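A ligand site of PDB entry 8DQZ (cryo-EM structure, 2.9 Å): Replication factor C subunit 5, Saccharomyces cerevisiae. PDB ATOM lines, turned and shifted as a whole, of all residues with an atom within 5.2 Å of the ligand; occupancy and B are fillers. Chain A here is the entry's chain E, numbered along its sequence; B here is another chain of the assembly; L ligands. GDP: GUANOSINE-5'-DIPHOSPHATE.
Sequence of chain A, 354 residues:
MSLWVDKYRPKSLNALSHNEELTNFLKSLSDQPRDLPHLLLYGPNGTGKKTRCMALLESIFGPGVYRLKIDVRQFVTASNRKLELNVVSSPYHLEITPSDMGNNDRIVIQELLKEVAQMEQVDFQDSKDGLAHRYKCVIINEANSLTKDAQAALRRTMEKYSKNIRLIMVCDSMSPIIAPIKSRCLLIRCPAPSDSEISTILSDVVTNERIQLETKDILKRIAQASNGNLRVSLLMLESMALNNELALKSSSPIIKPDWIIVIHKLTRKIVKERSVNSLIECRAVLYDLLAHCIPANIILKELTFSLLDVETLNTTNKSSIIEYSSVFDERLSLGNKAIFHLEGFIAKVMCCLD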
ATOM      1  N   VAL A   5     -13.808  15.473 -28.503  1.00  0.00           N
ATOM      2  CA  VAL A   5     -13.440  14.417 -27.571  1.00  0.00           C
ATOM      3  C   VAL A   5     -14.657  13.889 -26.838  1.00  0.00           C
ATOM      4  O   VAL A   5     -14.724  12.700 -26.487  1.00  0.00           O
ATOM      5  CB  VAL A   5     -12.360  14.922 -26.588  1.00  0.00           C
ATOM      6  CG1 VAL A   5     -12.964  15.946 -25.625  1.00  0.00           C
ATOM      7  CG2 VAL A   5     -11.748  13.765 -25.824  1.00  0.00           C
ATOM      8  N   ASP A   6     -15.650  14.752 -26.585  1.00  0.00           N
ATOM      9  CA  ASP A   6     -16.843  14.373 -25.845  1.00  0.00           C
ATOM     10  C   ASP A   6     -18.044  14.076 -26.734  1.00  0.00           C
ATOM     11  O   ASP A   6     -18.919  13.310 -26.330  1.00  0.00           O
ATOM     12  CB  ASP A   6     -17.223  15.477 -24.850  1.00  0.00           C
ATOM     13  CG  ASP A   6     -16.271  15.560 -23.677  1.00  0.00           C
ATOM     14  OD1 ASP A   6     -15.915  14.505 -23.122  1.00  0.00           O
ATOM     15  OD2 ASP A   6     -15.878  16.688 -23.321  1.00  0.00           O
ATOM     16  N   TYR A   8     -18.123  12.435 -29.580  1.00  0.00           N
ATOM     17  CA  TYR A   8     -18.024  11.158 -30.278  1.00  0.00           C
ATOM     18  C   TYR A   8     -17.591  10.041 -29.336  1.00  0.00           C
ATOM     19  O   TYR A   8     -17.006   9.048 -29.766  1.00  0.00           O
ATOM     20  CB  TYR A   8     -17.048  11.271 -31.448  1.00  0.00           C
ATOM     21  CG  TYR A   8     -17.462  12.289 -32.488  1.00  0.00           C
ATOM     22  CD1 TYR A   8     -18.368  11.955 -33.487  1.00  0.00           C
ATOM     23  CD2 TYR A   8     -16.949  13.577 -32.469  1.00  0.00           C
ATOM     24  CE1 TYR A   8     -18.747  12.881 -34.441  1.00  0.00           C
ATOM     25  CE2 TYR A   8     -17.330  14.510 -33.416  1.00  0.00           C
ATOM     26  CZ  TYR A   8     -18.226  14.155 -34.395  1.00  0.00           C
ATOM     27  OH  TYR A   8     -18.606  15.081 -35.350  1.00  0.00           O
ATOM     28  N   ARG A   9     -17.887  10.174 -28.051  1.00  0.00           N
ATOM     29  CA  ARG A   9     -17.552   9.135 -27.085  1.00  0.00           C
ATOM     30  C   ARG A   9     -18.545   7.994 -27.199  1.00  0.00           C
ATOM     31  O   ARG A   9     -19.754   8.223 -27.132  1.00  0.00           O
ATOM     32  CB  ARG A   9     -17.549   9.701 -25.665  1.00  0.00           C
ATOM     33  CG  ARG A   9     -17.235   8.671 -24.602  1.00  0.00           C
ATOM     34  CD  ARG A   9     -17.003   9.324 -23.237  1.00  0.00           C
ATOM     35  NE  ARG A   9     -18.003  10.346 -22.950  1.00  0.00           N
ATOM     36  CZ  ARG A   9     -17.745  11.625 -22.722  1.00  0.00           C
ATOM     37  NH1 ARG A   9     -16.512  12.101 -22.735  1.00  0.00           N
ATOM     38  NH2 ARG A   9     -18.760  12.459 -22.472  1.00  0.00           N
ATOM     39  N   PRO A  10     -18.091   6.745 -27.371  1.00  0.00           N
ATOM     40  CA  PRO A  10     -19.037   5.633 -27.464  1.00  0.00           C
ATOM     41  C   PRO A  10     -19.859   5.495 -26.182  1.00  0.00           C
ATOM     42  O   PRO A  10     -19.355   5.704 -25.082  1.00  0.00           O
ATOM     43  CB  PRO A  10     -18.130   4.410 -27.683  1.00  0.00           C
ATOM     44  CG  PRO A  10     -16.806   4.819 -27.154  1.00  0.00           C
ATOM     45  CD  PRO A  10     -16.693   6.278 -27.429  1.00  0.00           C
ATOM     46  N   ALA A  15     -19.983  -0.047 -29.169  1.00  0.00           N
ATOM     47  CA  ALA A  15     -19.406   1.095 -29.857  1.00  0.00           C
ATOM     48  C   ALA A  15     -17.912   1.258 -29.609  1.00  0.00           C
ATOM     49  O   ALA A  15     -17.287   2.154 -30.180  1.00  0.00           O
ATOM     50  CB  ALA A  15     -20.136   2.377 -29.449  1.00  0.00           C
ATOM     51  N   LEU A  16     -17.321   0.417 -28.764  1.00  0.00           N
ATOM     52  CA  LEU A  16     -15.888   0.497 -28.480  1.00  0.00           C
ATOM     53  C   LEU A  16     -15.101  -0.033 -29.662  1.00  0.00           C
ATOM     54  O   LEU A  16     -15.411  -1.106 -30.200  1.00  0.00           O
ATOM     55  CB  LEU A  16     -15.554  -0.287 -27.215  1.00  0.00           C
ATOM     56  CG  LEU A  16     -16.347   0.103 -25.964  1.00  0.00           C
ATOM     57  CD1 LEU A  16     -15.934  -0.762 -24.777  1.00  0.00           C
ATOM     58  CD2 LEU A  16     -16.161   1.574 -25.634  1.00  0.00           C
ATOM     59  N   SER A  17     -14.072   0.716 -30.068  1.00  0.00           N
ATOM     60  CA  SER A  17     -13.278   0.359 -31.240  1.00  0.00           C
ATOM     61  C   SER A  17     -12.037  -0.435 -30.873  1.00  0.00           C
ATOM     62  O   SER A  17     -11.844  -1.571 -31.332  1.00  0.00           O
ATOM     63  CB  SER A  17     -12.893   1.623 -32.011  1.00  0.00           C
ATOM     64  OG  SER A  17     -14.046   2.291 -32.509  1.00  0.00           O
ATOM     65  N   HIS A  18     -11.171   0.136 -30.035  1.00  0.00           N
ATOM     66  CA  HIS A  18      -9.898  -0.482 -29.697  1.00  0.00           C
ATOM     67  C   HIS A  18     -10.053  -1.430 -28.511  1.00  0.00           C
ATOM     68  O   HIS A  18     -11.026  -1.379 -27.754  1.00  0.00           O
ATOM     69  CB  HIS A  18      -8.851   0.588 -29.377  1.00  0.00           C
ATOM     70  CG  HIS A  18      -9.143   1.376 -28.144  1.00  0.00           C
ATOM     71  ND1 HIS A  18      -8.496   1.148 -26.945  1.00  0.00           N
ATOM     72  CD2 HIS A  18     -10.001   2.397 -27.915  1.00  0.00           C
ATOM     73  CE1 HIS A  18      -8.939   1.990 -26.038  1.00  0.00           C
ATOM     74  NE2 HIS A  18      -9.858   2.756 -26.599  1.00  0.00           N
ATOM     75  N   PRO A  44      -3.361   3.027 -18.111  1.00  0.00           N
ATOM     76  CA  PRO A  44      -2.870   4.380 -18.381  1.00  0.00           C
ATOM     77  C   PRO A  44      -4.008   5.379 -18.510  1.00  0.00           C
ATOM     78  O   PRO A  44      -5.134   5.048 -18.889  1.00  0.00           O
ATOM     79  CB  PRO A  44      -2.114   4.223 -19.708  1.00  0.00           C
ATOM     80  CG  PRO A  44      -1.780   2.771 -19.787  1.00  0.00           C
ATOM     81  CD  PRO A  44      -2.927   2.063 -19.140  1.00  0.00           C
ATOM     82  N   ASN A  45      -3.701   6.628 -18.167  1.00  0.00           N
ATOM     83  CA  ASN A  45      -4.686   7.697 -18.254  1.00  0.00           C
ATOM     84  C   ASN A  45      -5.056   7.974 -19.709  1.00  0.00           C
ATOM     85  O   ASN A  45      -4.247   7.836 -20.629  1.00  0.00           O
ATOM     86  CB  ASN A  45      -4.141   8.973 -17.604  1.00  0.00           C
ATOM     87  CG  ASN A  45      -4.305   8.971 -16.098  1.00  0.00           C
ATOM     88  OD1 ASN A  45      -5.412   9.121 -15.583  1.00  0.00           O
ATOM     89  ND2 ASN A  45      -3.196   8.803 -15.390  1.00  0.00           N
ATOM     90  N   GLY A  46      -6.303   8.389 -19.905  1.00  0.00           N
ATOM     91  CA  GLY A  46      -6.770   8.753 -21.236  1.00  0.00           C
ATOM     92  C   GLY A  46      -6.958   7.586 -22.181  1.00  0.00           C
ATOM     93  O   GLY A  46      -6.935   7.783 -23.397  1.00  0.00           O
ATOM     94  N   THR A  47      -7.153   6.380 -21.660  1.00  0.00           N
ATOM     95  CA  THR A  47      -7.316   5.190 -22.488  1.00  0.00           C
ATOM     96  C   THR A  47      -8.771   4.798 -22.704  1.00  0.00           C
ATOM     97  O   THR A  47      -9.088   4.144 -23.706  1.00  0.00           O
ATOM     98  CB  THR A  47      -6.566   4.006 -21.867  1.00  0.00           C
ATOM     99  OG1 THR A  47      -7.041   3.778 -20.533  1.00  0.00           O
ATOM    100  CG2 THR A  47      -5.077   4.280 -21.838  1.00  0.00           C
ATOM    101  N   GLY A  48      -9.665   5.185 -21.788  1.00  0.00           N
ATOM    102  CA  GLY A  48     -11.077   4.855 -21.930  1.00  0.00           C
ATOM    103  C   GLY A  48     -11.599   3.991 -20.794  1.00  0.00           C
ATOM    104  O   GLY A  48     -12.566   3.244 -20.984  1.00  0.00           O
ATOM    105  N   LYS A  49     -10.968   4.080 -19.622  1.00  0.00           N
ATOM    106  CA  LYS A  49     -11.415   3.279 -18.490  1.00  0.00           C
ATOM    107  C   LYS A  49     -12.805   3.668 -18.042  1.00  0.00           C
ATOM    108  O   LYS A  49     -13.681   2.813 -17.854  1.00  0.00           O
ATOM    109  CB  LYS A  49     -10.422   3.422 -17.336  1.00  0.00           C
ATOM    110  CG  LYS A  49      -8.995   3.000 -17.683  1.00  0.00           C
ATOM    111  CD  LYS A  49      -8.095   2.980 -16.454  1.00  0.00           C
ATOM    112  CE  LYS A  49      -7.806   4.384 -15.941  1.00  0.00           C
ATOM    113  NZ  LYS A  49      -7.002   5.180 -16.906  1.00  0.00           N
ATOM    114  N   LYS A  50     -13.042   4.973 -17.858  1.00  0.00           N
ATOM    115  CA  LYS A  50     -14.363   5.432 -17.434  1.00  0.00           C
ATOM    116  C   LYS A  50     -15.418   5.158 -18.509  1.00  0.00           C
ATOM    117  O   LYS A  50     -16.560   4.826 -18.192  1.00  0.00           O
ATOM    118  CB  LYS A  50     -14.319   6.916 -17.097  1.00  0.00           C
ATOM    119  CG  LYS A  50     -15.598   7.471 -16.455  1.00  0.00           C
ATOM    120  CD  LYS A  50     -15.978   6.719 -15.181  1.00  0.00           C
ATOM    121  CE  LYS A  50     -17.263   7.251 -14.560  1.00  0.00           C
ATOM    122  NZ  LYS A  50     -17.509   8.690 -14.860  1.00  0.00           N
ATOM    123  N   THR A  51     -15.042   5.297 -19.780  1.00  0.00           N
ATOM    124  CA  THR A  51     -15.967   4.984 -20.854  1.00  0.00           C
ATOM    125  C   THR A  51     -16.377   3.517 -20.806  1.00  0.00           C
ATOM    126  O   THR A  51     -17.558   3.190 -20.969  1.00  0.00           O
ATOM    127  CB  THR A  51     -15.341   5.323 -22.209  1.00  0.00           C
ATOM    128  OG1 THR A  51     -15.120   6.731 -22.301  1.00  0.00           O
ATOM    129  CG2 THR A  51     -16.242   4.881 -23.354  1.00  0.00           C
ATOM    130  N   ARG A  52     -15.410   2.619 -20.592  1.00  0.00           N
ATOM    131  CA  ARG A  52     -15.736   1.206 -20.498  1.00  0.00           C
ATOM    132  C   ARG A  52     -16.575   0.903 -19.275  1.00  0.00           C
ATOM    133  O   ARG A  52     -17.478   0.063 -19.318  1.00  0.00           O
ATOM    134  CB  ARG A  52     -14.449   0.377 -20.481  1.00  0.00           C
ATOM    135  CG  ARG A  52     -13.953   0.019 -21.873  1.00  0.00           C
ATOM    136  CD  ARG A  52     -12.453  -0.177 -21.912  1.00  0.00           C
ATOM    137  NE  ARG A  52     -11.977  -0.372 -23.276  1.00  0.00           N
ATOM    138  CZ  ARG A  52     -11.904   0.589 -24.191  1.00  0.00           C
ATOM    139  NH1 ARG A  52     -12.267   1.831 -23.918  1.00  0.00           N
ATOM    140  NH2 ARG A  52     -11.465   0.282 -25.408  1.00  0.00           N
ATOM    141  N   ILE A 201      -9.541   6.357 -35.190  1.00  0.00           N
ATOM    142  CA  ILE A 201     -10.524   7.192 -34.495  1.00  0.00           C
ATOM    143  C   ILE A 201     -10.422   8.638 -34.947  1.00  0.00           C
ATOM    144  O   ILE A 201     -11.431   9.313 -35.174  1.00  0.00           O
ATOM    145  CB  ILE A 201     -10.350   7.053 -32.964  1.00  0.00           C
ATOM    146  CG1 ILE A 201     -10.605   5.610 -32.525  1.00  0.00           C
ATOM    147  CG2 ILE A 201     -11.277   8.017 -32.239  1.00  0.00           C
ATOM    148  CD1 ILE A 201     -10.102   5.291 -31.134  1.00  0.00           C
ATOM    149  N   LEU A 230      -5.611   8.923 -25.551  1.00  0.00           N
ATOM    150  CA  LEU A 230      -6.584   9.198 -26.613  1.00  0.00           C
ATOM    151  C   LEU A 230      -7.242  10.550 -26.430  1.00  0.00           C
ATOM    152  O   LEU A 230      -7.490  11.261 -27.415  1.00  0.00           O
ATOM    153  CB  LEU A 230      -7.641   8.090 -26.646  1.00  0.00           C
ATOM    154  CG  LEU A 230      -8.671   8.163 -27.768  1.00  0.00           C
ATOM    155  CD1 LEU A 230      -8.004   8.218 -29.135  1.00  0.00           C
ATOM    156  CD2 LEU A 230      -9.607   6.968 -27.692  1.00  0.00           C
ATOM    157  N   ARG A 231      -7.535  10.941 -25.183  1.00  0.00           N
ATOM    158  CA  ARG A 231      -8.109  12.257 -24.941  1.00  0.00           C
ATOM    159  C   ARG A 231      -7.166  13.356 -25.413  1.00  0.00           C
ATOM    160  O   ARG A 231      -7.599  14.324 -26.051  1.00  0.00           O
ATOM    161  CB  ARG A 231      -8.411  12.434 -23.454  1.00  0.00           C
ATOM    162  CG  ARG A 231      -8.743  13.863 -23.046  1.00  0.00           C
ATOM    163  CD  ARG A 231      -9.319  13.932 -21.641  1.00  0.00           C
ATOM    164  NE  ARG A 231      -8.481  13.268 -20.658  1.00  0.00           N
ATOM    165  CZ  ARG A 231      -8.667  12.039 -20.196  1.00  0.00           C
ATOM    166  NH1 ARG A 231      -9.676  11.287 -20.615  1.00  0.00           N
ATOM    167  NH2 ARG A 231      -7.824  11.546 -19.297  1.00  0.00           N
ATOM    168  N   LEU A 234      -7.273  13.499 -29.257  1.00  0.00           N
ATOM    169  CA  LEU A 234      -8.474  14.133 -29.799  1.00  0.00           C
ATOM    170  C   LEU A 234      -8.454  15.639 -29.579  1.00  0.00           C
ATOM    171  O   LEU A 234      -8.766  16.413 -30.497  1.00  0.00           O
ATOM    172  CB  LEU A 234      -9.713  13.506 -29.158  1.00  0.00           C
ATOM    173  CG  LEU A 234      -9.957  12.033 -29.521  1.00  0.00           C
ATOM    174  CD1 LEU A 234     -10.873  11.368 -28.501  1.00  0.00           C
ATOM    175  CD2 LEU A 234     -10.532  11.903 -30.917  1.00  0.00           C
ATOM    176  N   SER B 695     -15.578  13.658 -19.563  1.00  0.00           N
ATOM    177  CA  SER B 695     -15.164  12.400 -18.928  1.00  0.00           C
ATOM    178  C   SER B 695     -13.705  12.548 -18.525  1.00  0.00           C
ATOM    179  O   SER B 695     -12.803  12.199 -19.299  1.00  0.00           O
ATOM    180  CB  SER B 695     -15.389  11.219 -19.869  1.00  0.00           C
ATOM    181  OG  SER B 695     -15.070   9.996 -19.226  1.00  0.00           O
ATOM    182  N   THR B 696     -13.471  13.064 -17.320  1.00  0.00           N
ATOM    183  CA  THR B 696     -12.116  13.299 -16.835  1.00  0.00           C
ATOM    184  C   THR B 696     -12.216  13.746 -15.380  1.00  0.00           C
ATOM    185  O   THR B 696     -13.303  13.885 -14.826  1.00  0.00           O
ATOM    186  CB  THR B 696     -11.379  14.347 -17.671  1.00  0.00           C
ATOM    187  OG1 THR B 696     -10.211  14.789 -16.967  1.00  0.00           O
ATOM    188  CG2 THR B 696     -12.284  15.544 -17.939  1.00  0.00           C
ATOM    189  N   TYR B 705      -8.218  19.686 -21.116  1.00  0.00           N
ATOM    190  CA  TYR B 705      -9.392  20.353 -21.683  1.00  0.00           C
ATOM    191  C   TYR B 705      -9.200  21.865 -21.804  1.00  0.00           C
ATOM    192  O   TYR B 705      -9.566  22.442 -22.824  1.00  0.00           O
ATOM    193  CB  TYR B 705     -10.624  20.043 -20.836  1.00  0.00           C
ATOM    194  CG  TYR B 705     -11.359  18.793 -21.271  1.00  0.00           C
ATOM    195  CD1 TYR B 705     -12.311  18.839 -22.277  1.00  0.00           C
ATOM    196  CD2 TYR B 705     -11.091  17.571 -20.677  1.00  0.00           C
ATOM    197  CE1 TYR B 705     -12.982  17.697 -22.676  1.00  0.00           C
ATOM    198  CE2 TYR B 705     -11.759  16.422 -21.070  1.00  0.00           C
ATOM    199  CZ  TYR B 705     -12.698  16.495 -22.071  1.00  0.00           C
ATOM    200  OH  TYR B 705     -13.369  15.353 -22.470  1.00  0.00           O
HETATM  201  PB  GDP L   1      -9.728   7.707 -18.653  1.00  0.00           P
HETATM  202  O1B GDP L   1      -9.168   6.324 -18.851  1.00  0.00           O
HETATM  203  O2B GDP L   1     -10.928   7.642 -17.749  1.00  0.00           O
HETATM  204  O3B GDP L   1      -8.665   8.582 -18.025  1.00  0.00           O
HETATM  205  O3A GDP L   1     -10.164   8.336 -20.105  1.00  0.00           O
HETATM  206  PA  GDP L   1     -11.715   8.392 -20.662  1.00  0.00           P
HETATM  207  O1A GDP L   1     -12.426   7.101 -20.293  1.00  0.00           O
HETATM  208  O2A GDP L   1     -12.442   9.547 -20.021  1.00  0.00           O
HETATM  209  O5' GDP L   1     -11.714   8.567 -22.304  1.00  0.00           O
HETATM  210  C5' GDP L   1     -11.353   9.813 -22.835  1.00  0.00           C
HETATM  211  C4' GDP L   1     -11.877   9.933 -24.256  1.00  0.00           C
HETATM  212  O4' GDP L   1     -11.325   8.691 -25.129  1.00  0.00           O
HETATM  213  C3' GDP L   1     -13.182   9.869 -24.280  1.00  0.00           C
HETATM  214  O3' GDP L   1     -13.756  11.244 -24.345  1.00  0.00           O
HETATM  215  C2' GDP L   1     -13.540   9.093 -25.557  1.00  0.00           C
HETATM  216  O2' GDP L   1     -13.941   9.947 -26.531  1.00  0.00           O
HETATM  217  C1' GDP L   1     -12.246   8.365 -25.990  1.00  0.00           C
HETATM  218  N9  GDP L   1     -12.448   6.907 -25.959  1.00  0.00           N
HETATM  219  C8  GDP L   1     -12.325   6.047 -24.929  1.00  0.00           C
HETATM  220  N7  GDP L   1     -12.604   4.817 -25.404  1.00  0.00           N
HETATM  221  C5  GDP L   1     -12.905   4.927 -26.701  1.00  0.00           C
HETATM  222  C6  GDP L   1     -13.295   3.871 -27.750  1.00  0.00           C
HETATM  223  O6  GDP L   1     -13.385   2.731 -27.444  1.00  0.00           O
HETATM  224  N1  GDP L   1     -13.558   4.282 -29.104  1.00  0.00           N
HETATM  225  C2  GDP L   1     -13.445   5.673 -29.466  1.00  0.00           C
HETATM  226  N2  GDP L   1     -13.710   6.091 -30.826  1.00  0.00           N
HETATM  227  N3  GDP L   1     -13.072   6.667 -28.459  1.00  0.00           N
HETATM  228  C4  GDP L   1     -12.795   6.235 -27.057  1.00  0.00           C
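NZ of Lys 49 is in hydrogen-bond range of O of Pro 44 (2.7 Å).
The backbone NH of Leu 230 sits at hydrogen-bond distance from the backbone carbonyl oxygen of Gly 46.
The backbone carbonyl oxygen of Gly 48 lies within hydrogen-bond range of the guanidinium group of Arg 52.
The guanidinium group of Arg 9 lies within salt-bridge range of the side-chain carboxylate of Asp 6 (2.5 Å).
O of His 18 lies within hydrogen-bond range of NH2 of Arg 52 (2.9 Å).
NE2 of His 18 sits close to O of Thr 47, 3.3 Å away.
The backbone carbonyl oxygen of Pro 44 sits at hydrogen-bond distance from the side-chain hydroxyl of Thr 47.
Pro 10 touches the ligand.
Leu 16 touches the ligand (CD2 to O6, 3.5 Å).
His 18 touches the ligand (CD2 to O6, 3.4 Å).
Ile 201 touches the ligand (CG2 to N2, 3.4 Å).
CD2 of Leu 230 touches N9 of the ligand, at 3.3 Å.
Leu 234 touches the ligand.
An oxygen (O3') of the ligand is in hydrogen-bond range of the backbone carbonyl oxygen (O) of Val 5 (2.8 Å).
The backbone carbonyl oxygen (O) of Ser 695 of chain B sits close to an oxygen (O2A) of the ligand (2.8 Å).
An oxygen (O2A) of the ligand is in hydrogen-bond range of the side-chain hydroxyl (OG) of Ser 695 of chain B, 2.8 Å away.
O1B of the ligand sits at hydrogen-bond distance from N of Lys 49 (3.0 Å).
NZ of Lys 49 lies within salt-bridge range of O1B of the ligand (3.1 Å).
N of Gly 46 sits at hydrogen-bond distance from O3B of the ligand.
The guanidinium group of Arg 231 lies within salt-bridge range of an oxygen (O2A) of the ligand (3.3 Å).
The backbone NH (N) of Gly 48 sits at hydrogen-bond distance from an oxygen (O1B) of the ligand, at 3.2 Å.
The backbone NH (N) of Thr 51 lies within hydrogen-bond range of an oxygen (O1A) of the ligand.
O1A of the ligand sits at hydrogen-bond distance from OG1 of Thr 51 (3.4 Å).
The backbone NH of Lys 50 lies within hydrogen-bond range of an oxygen (O1A) of the ligand, 3.3 Å away.
NH1 of Arg 9 is in hydrogen-bond range of O3' of the ligand (3.3 Å).
The guanidinium group of Arg 52 is in hydrogen-bond range of a nitrogen (N7) of the ligand, at 3.4 Å.
N of Ser 17 is in hydrogen-bond range of O6 of the ligand, at 3.4 Å.
O1B of the ligand lies within hydrogen-bond range of N of Thr 47.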
